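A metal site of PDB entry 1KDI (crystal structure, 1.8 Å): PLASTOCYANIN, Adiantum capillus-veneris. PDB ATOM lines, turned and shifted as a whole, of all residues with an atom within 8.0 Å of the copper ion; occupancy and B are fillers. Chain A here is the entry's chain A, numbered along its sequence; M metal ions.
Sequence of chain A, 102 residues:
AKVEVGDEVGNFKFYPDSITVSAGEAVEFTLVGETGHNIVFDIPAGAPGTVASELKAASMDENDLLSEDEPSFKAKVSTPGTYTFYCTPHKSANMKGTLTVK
The copper ion is bound by a ring nitrogen (ND1) of His 37 (2.0 Å), a ring nitrogen (ND1) of His 90 (2.1 Å) and the side-chain sulfur of Cys 87 (2.2 Å). The copper ion has three donor atoms within binding distance. Slightly farther from the copper ion lies SD of Met 95 (2.9 Å).
The backbone NH (N) of Asn 38 sits close to the side-chain sulfur (SG) of Cys 87, at 3.5 Å. The backbone NH (N) of Met 95 lies within hydrogen-bond range of the backbone carbonyl oxygen (O) of His 90 (3.4 Å). N of Lys 13 lies within hydrogen-bond range of SD of Met 95 (3.7 Å). O of Met 95 is in hydrogen-bond range of N of Cys 87, at 3.1 Å. A ring nitrogen (ND1) of His 37 lies close to the side-chain sulfur of Met 95, at 3.2 Å.
Four residues have an atom within 4 Å of the copper ion: His 37, Cys 87, His 90 and Met 95. The nearest printed residue that does not touch the copper ion is Gly 36 (4.1 Å).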
ATOM      1  N   VAL A   5      13.188  17.298  -6.692  1.00  0.00           N
ATOM      2  CA  VAL A   5      14.378  18.067  -6.428  1.00  0.00           C
ATOM      3  C   VAL A   5      15.271  17.974  -7.683  1.00  0.00           C
ATOM      4  O   VAL A   5      15.752  16.889  -7.996  1.00  0.00           O
ATOM      5  CB  VAL A   5      15.120  17.477  -5.203  1.00  0.00           C
ATOM      6  CG1 VAL A   5      16.291  18.368  -4.867  1.00  0.00           C
ATOM      7  CG2 VAL A   5      14.183  17.390  -4.001  1.00  0.00           C
ATOM      8  N   GLY A   6      15.430  19.108  -8.352  1.00  0.00           N
ATOM      9  CA  GLY A   6      16.177  19.199  -9.607  1.00  0.00           C
ATOM     10  C   GLY A   6      15.372  18.628 -10.758  1.00  0.00           C
ATOM     11  O   GLY A   6      14.216  18.232 -10.647  1.00  0.00           O
ATOM     12  N   ASN A  11      19.017  22.046 -13.665  1.00  0.00           N
ATOM     13  CA  ASN A  11      18.580  23.337 -13.118  1.00  0.00           C
ATOM     14  C   ASN A  11      18.508  23.157 -11.618  1.00  0.00           C
ATOM     15  O   ASN A  11      18.164  22.085 -11.138  1.00  0.00           O
ATOM     16  CB  ASN A  11      17.152  23.801 -13.491  1.00  0.00           C
ATOM     17  CG  ASN A  11      17.069  24.234 -14.925  1.00  0.00           C
ATOM     18  OD1 ASN A  11      17.772  25.145 -15.368  1.00  0.00           O
ATOM     19  ND2 ASN A  11      16.232  23.616 -15.736  1.00  0.00           N
ATOM     20  N   PHE A  12      18.824  24.192 -10.868  1.00  0.00           N
ATOM     21  CA  PHE A  12      18.885  24.120  -9.416  1.00  0.00           C
ATOM     22  C   PHE A  12      17.554  24.643  -8.866  1.00  0.00           C
ATOM     23  O   PHE A  12      17.432  25.795  -8.438  1.00  0.00           O
ATOM     24  CB  PHE A  12      20.042  24.970  -8.987  1.00  0.00           C
ATOM     25  CG  PHE A  12      21.417  24.679  -9.611  1.00  0.00           C
ATOM     26  CD1 PHE A  12      21.827  23.404  -9.897  1.00  0.00           C
ATOM     27  CD2 PHE A  12      22.254  25.749  -9.863  1.00  0.00           C
ATOM     28  CE1 PHE A  12      23.092  23.189 -10.423  1.00  0.00           C
ATOM     29  CE2 PHE A  12      23.517  25.524 -10.388  1.00  0.00           C
ATOM     30  CZ  PHE A  12      23.931  24.250 -10.660  1.00  0.00           C
ATOM     31  N   LYS A  13      16.539  23.784  -8.930  1.00  0.00           N
ATOM     32  CA  LYS A  13      15.178  24.096  -8.501  1.00  0.00           C
ATOM     33  C   LYS A  13      14.441  22.954  -7.862  1.00  0.00           C
ATOM     34  O   LYS A  13      14.618  21.773  -8.171  1.00  0.00           O
ATOM     35  CB  LYS A  13      14.319  24.555  -9.689  1.00  0.00           C
ATOM     36  CG  LYS A  13      14.513  25.981 -10.097  1.00  0.00           C
ATOM     37  CD  LYS A  13      13.671  26.294 -11.297  1.00  0.00           C
ATOM     38  CE  LYS A  13      14.126  27.639 -11.843  1.00  0.00           C
ATOM     39  NZ  LYS A  13      13.446  27.912 -13.105  1.00  0.00           N
ATOM     40  N   PHE A  14      13.533  23.401  -6.994  1.00  0.00           N
ATOM     41  CA  PHE A  14      12.521  22.523  -6.363  1.00  0.00           C
ATOM     42  C   PHE A  14      11.229  22.641  -7.193  1.00  0.00           C
ATOM     43  O   PHE A  14      10.885  23.739  -7.633  1.00  0.00           O
ATOM     44  CB  PHE A  14      12.160  22.949  -4.928  1.00  0.00           C
ATOM     45  CG  PHE A  14      13.334  22.684  -4.000  1.00  0.00           C
ATOM     46  CD1 PHE A  14      13.582  21.386  -3.568  1.00  0.00           C
ATOM     47  CD2 PHE A  14      14.152  23.745  -3.595  1.00  0.00           C
ATOM     48  CE1 PHE A  14      14.659  21.158  -2.727  1.00  0.00           C
ATOM     49  CE2 PHE A  14      15.221  23.487  -2.765  1.00  0.00           C
ATOM     50  CZ  PHE A  14      15.464  22.210  -2.340  1.00  0.00           C
ATOM     51  N   LEU A  31      14.733  13.095  -5.708  1.00  0.00           N
ATOM     52  CA  LEU A  31      15.728  13.593  -6.646  1.00  0.00           C
ATOM     53  C   LEU A  31      15.355  13.237  -8.074  1.00  0.00           C
ATOM     54  O   LEU A  31      15.029  12.086  -8.319  1.00  0.00           O
ATOM     55  CB  LEU A  31      17.091  12.978  -6.365  1.00  0.00           C
ATOM     56  CG  LEU A  31      18.217  13.513  -7.244  1.00  0.00           C
ATOM     57  CD1 LEU A  31      18.549  14.928  -6.868  1.00  0.00           C
ATOM     58  CD2 LEU A  31      19.420  12.626  -7.091  1.00  0.00           C
ATOM     59  N   THR A  35      22.372  15.516 -10.822  1.00  0.00           N
ATOM     60  CA  THR A  35      22.924  16.462  -9.872  1.00  0.00           C
ATOM     61  C   THR A  35      22.353  16.155  -8.477  1.00  0.00           C
ATOM     62  O   THR A  35      21.146  16.016  -8.300  1.00  0.00           O
ATOM     63  CB  THR A  35      22.536  17.868 -10.346  1.00  0.00           C
ATOM     64  OG1 THR A  35      22.996  17.964 -11.687  1.00  0.00           O
ATOM     65  CG2 THR A  35      23.196  18.976  -9.572  1.00  0.00           C
ATOM     66  N   GLY A  36      23.253  15.977  -7.490  1.00  0.00           N
ATOM     67  CA  GLY A  36      22.900  15.726  -6.118  1.00  0.00           C
ATOM     68  C   GLY A  36      22.468  17.016  -5.462  1.00  0.00           C
ATOM     69  O   GLY A  36      22.904  18.143  -5.758  1.00  0.00           O
ATOM     70  N   HIS A  37      21.561  16.953  -4.503  1.00  0.00           N
ATOM     71  CA  HIS A  37      21.033  18.147  -3.839  1.00  0.00           C
ATOM     72  C   HIS A  37      20.660  17.697  -2.467  1.00  0.00           C
ATOM     73  O   HIS A  37      20.666  16.512  -2.197  1.00  0.00           O
ATOM     74  CB  HIS A  37      19.723  18.692  -4.474  1.00  0.00           C
ATOM     75  CG  HIS A  37      19.813  19.146  -5.941  1.00  0.00           C
ATOM     76  ND1 HIS A  37      20.274  20.327  -6.267  1.00  0.00           N
ATOM     77  CD2 HIS A  37      19.391  18.432  -7.031  1.00  0.00           C
ATOM     78  CE1 HIS A  37      20.148  20.390  -7.592  1.00  0.00           C
ATOM     79  NE2 HIS A  37      19.617  19.264  -8.018  1.00  0.00           N
ATOM     80  N   ASN A  38      20.390  18.617  -1.593  1.00  0.00           N
ATOM     81  CA  ASN A  38      19.761  18.215  -0.332  1.00  0.00           C
ATOM     82  C   ASN A  38      18.760  19.269   0.141  1.00  0.00           C
ATOM     83  O   ASN A  38      18.470  20.243  -0.585  1.00  0.00           O
ATOM     84  CB  ASN A  38      20.850  17.964   0.720  1.00  0.00           C
ATOM     85  CG  ASN A  38      21.546  19.125   1.364  1.00  0.00           C
ATOM     86  OD1 ASN A  38      21.432  20.311   1.042  1.00  0.00           O
ATOM     87  ND2 ASN A  38      22.349  18.757   2.328  1.00  0.00           N
ATOM     88  N   ILE A  39      18.166  19.068   1.317  1.00  0.00           N
ATOM     89  CA  ILE A  39      17.181  20.003   1.844  1.00  0.00           C
ATOM     90  C   ILE A  39      17.390  20.147   3.355  1.00  0.00           C
ATOM     91  O   ILE A  39      17.433  19.218   4.152  1.00  0.00           O
ATOM     92  CB  ILE A  39      15.695  19.505   1.395  1.00  0.00           C
ATOM     93  CG1 ILE A  39      14.763  19.524   2.547  1.00  0.00           C
ATOM     94  CG2 ILE A  39      15.664  18.105   0.793  1.00  0.00           C
ATOM     95  CD1 ILE A  39      14.244  20.900   2.658  1.00  0.00           C
ATOM     96  N   LEU A  65      23.815  14.164   0.644  1.00  0.00           N
ATOM     97  CA  LEU A  65      23.273  14.608  -0.626  1.00  0.00           C
ATOM     98  C   LEU A  65      22.391  13.487  -1.129  1.00  0.00           C
ATOM     99  O   LEU A  65      22.710  12.312  -0.912  1.00  0.00           O
ATOM    100  CB  LEU A  65      24.357  14.869  -1.693  1.00  0.00           C
ATOM    101  CG  LEU A  65      25.225  16.142  -1.670  1.00  0.00           C
ATOM    102  CD1 LEU A  65      26.209  16.135  -2.828  1.00  0.00           C
ATOM    103  CD2 LEU A  65      24.375  17.359  -1.852  1.00  0.00           C
ATOM    104  N   TYR A  86      16.201  25.126   1.763  1.00  0.00           N
ATOM    105  CA  TYR A  86      17.140  25.386   0.683  1.00  0.00           C
ATOM    106  C   TYR A  86      18.056  24.190   0.525  1.00  0.00           C
ATOM    107  O   TYR A  86      18.041  23.238   1.316  1.00  0.00           O
ATOM    108  CB  TYR A  86      17.935  26.675   0.988  1.00  0.00           C
ATOM    109  CG  TYR A  86      18.814  26.573   2.219  1.00  0.00           C
ATOM    110  CD1 TYR A  86      20.083  26.002   2.156  1.00  0.00           C
ATOM    111  CD2 TYR A  86      18.323  27.008   3.424  1.00  0.00           C
ATOM    112  CE1 TYR A  86      20.845  25.859   3.303  1.00  0.00           C
ATOM    113  CE2 TYR A  86      19.071  26.867   4.574  1.00  0.00           C
ATOM    114  CZ  TYR A  86      20.314  26.299   4.496  1.00  0.00           C
ATOM    115  OH  TYR A  86      21.029  26.154   5.662  1.00  0.00           O
ATOM    116  N   CYS A  87      18.781  24.205  -0.588  1.00  0.00           N
ATOM    117  CA  CYS A  87      19.704  23.130  -0.857  1.00  0.00           C
ATOM    118  C   CYS A  87      21.060  23.669  -0.398  1.00  0.00           C
ATOM    119  O   CYS A  87      21.373  24.782  -0.822  1.00  0.00           O
ATOM    120  CB  CYS A  87      19.694  22.811  -2.397  1.00  0.00           C
ATOM    121  SG  CYS A  87      21.101  21.775  -2.883  1.00  0.00           S
ATOM    122  N   THR A  88      21.888  23.007   0.398  1.00  0.00           N
ATOM    123  CA  THR A  88      23.210  23.559   0.719  1.00  0.00           C
ATOM    124  C   THR A  88      24.190  23.752  -0.478  1.00  0.00           C
ATOM    125  O   THR A  88      24.658  24.887  -0.628  1.00  0.00           O
ATOM    126  CB  THR A  88      23.799  22.663   1.780  1.00  0.00           C
ATOM    127  OG1 THR A  88      22.895  22.560   2.864  1.00  0.00           O
ATOM    128  CG2 THR A  88      25.075  23.237   2.280  1.00  0.00           C
ATOM    129  N   PRO A  89      24.535  22.845  -1.416  1.00  0.00           N
ATOM    130  CA  PRO A  89      25.405  23.150  -2.567  1.00  0.00           C
ATOM    131  C   PRO A  89      25.015  24.364  -3.382  1.00  0.00           C
ATOM    132  O   PRO A  89      25.863  25.189  -3.749  1.00  0.00           O
ATOM    133  CB  PRO A  89      25.403  21.935  -3.442  1.00  0.00           C
ATOM    134  CG  PRO A  89      25.079  20.829  -2.511  1.00  0.00           C
ATOM    135  CD  PRO A  89      24.153  21.436  -1.471  1.00  0.00           C
ATOM    136  N   HIS A  90      23.684  24.525  -3.575  1.00  0.00           N
ATOM    137  CA  HIS A  90      23.228  25.513  -4.530  1.00  0.00           C
ATOM    138  C   HIS A  90      22.417  26.595  -3.881  1.00  0.00           C
ATOM    139  O   HIS A  90      21.675  27.316  -4.556  1.00  0.00           O
ATOM    140  CB  HIS A  90      22.397  24.848  -5.632  1.00  0.00           C
ATOM    141  CG  HIS A  90      23.103  23.686  -6.315  1.00  0.00           C
ATOM    142  ND1 HIS A  90      22.682  22.445  -6.142  1.00  0.00           N
ATOM    143  CD2 HIS A  90      24.209  23.746  -7.099  1.00  0.00           C
ATOM    144  CE1 HIS A  90      23.519  21.691  -6.822  1.00  0.00           C
ATOM    145  NE2 HIS A  90      24.395  22.485  -7.377  1.00  0.00           N
ATOM    146  N   LYS A  91      22.654  26.788  -2.584  1.00  0.00           N
ATOM    147  CA  LYS A  91      21.982  27.831  -1.801  1.00  0.00           C
ATOM    148  C   LYS A  91      22.275  29.179  -2.466  1.00  0.00           C
ATOM    149  O   LYS A  91      21.401  30.028  -2.608  1.00  0.00           O
ATOM    150  CB  LYS A  91      22.495  27.854  -0.349  1.00  0.00           C
ATOM    151  CG  LYS A  91      21.788  28.824   0.579  1.00  0.00           C
ATOM    152  CD  LYS A  91      22.592  28.993   1.881  1.00  0.00           C
ATOM    153  CE  LYS A  91      22.094  30.143   2.782  1.00  0.00           C
ATOM    154  NZ  LYS A  91      21.131  29.718   3.795  1.00  0.00           N
ATOM    155  N   ALA A  93      22.696  29.700  -5.588  1.00  0.00           N
ATOM    156  CA  ALA A  93      21.942  29.763  -6.821  1.00  0.00           C
ATOM    157  C   ALA A  93      20.437  29.924  -6.624  1.00  0.00           C
ATOM    158  O   ALA A  93      19.645  29.686  -7.546  1.00  0.00           O
ATOM    159  CB  ALA A  93      22.196  28.494  -7.644  1.00  0.00           C
ATOM    160  N   MET A  95      18.374  28.182  -4.919  1.00  0.00           N
ATOM    161  CA  MET A  95      17.668  26.930  -4.898  1.00  0.00           C
ATOM    162  C   MET A  95      17.039  26.794  -3.496  1.00  0.00           C
ATOM    163  O   MET A  95      17.636  26.337  -2.495  1.00  0.00           O
ATOM    164  CB  MET A  95      18.658  25.818  -5.226  1.00  0.00           C
ATOM    165  CG  MET A  95      17.890  24.533  -5.224  1.00  0.00           C
ATOM    166  SD  MET A  95      18.647  23.114  -5.973  1.00  0.00           S
ATOM    167  CE  MET A  95      17.378  21.902  -5.864  1.00  0.00           C
ATOM    168  N   LYS A  96      15.784  27.259  -3.453  1.00  0.00           N
ATOM    169  CA  LYS A  96      14.991  27.304  -2.237  1.00  0.00           C
ATOM    170  C   LYS A  96      13.489  27.235  -2.455  1.00  0.00           C
ATOM    171  O   LYS A  96      13.003  27.534  -3.550  1.00  0.00           O
ATOM    172  CB  LYS A  96      15.307  28.552  -1.490  1.00  0.00           C
ATOM    173  CG  LYS A  96      14.949  29.855  -2.150  1.00  0.00           C
ATOM    174  CD  LYS A  96      15.254  30.795  -1.004  1.00  0.00           C
ATOM    175  CE  LYS A  96      14.739  32.189  -1.268  1.00  0.00           C
ATOM    176  NZ  LYS A  96      14.856  32.912  -0.017  1.00  0.00           N
HETATM  177 CU    CU M   1      21.031  21.690  -5.085  1.00  0.00          CU
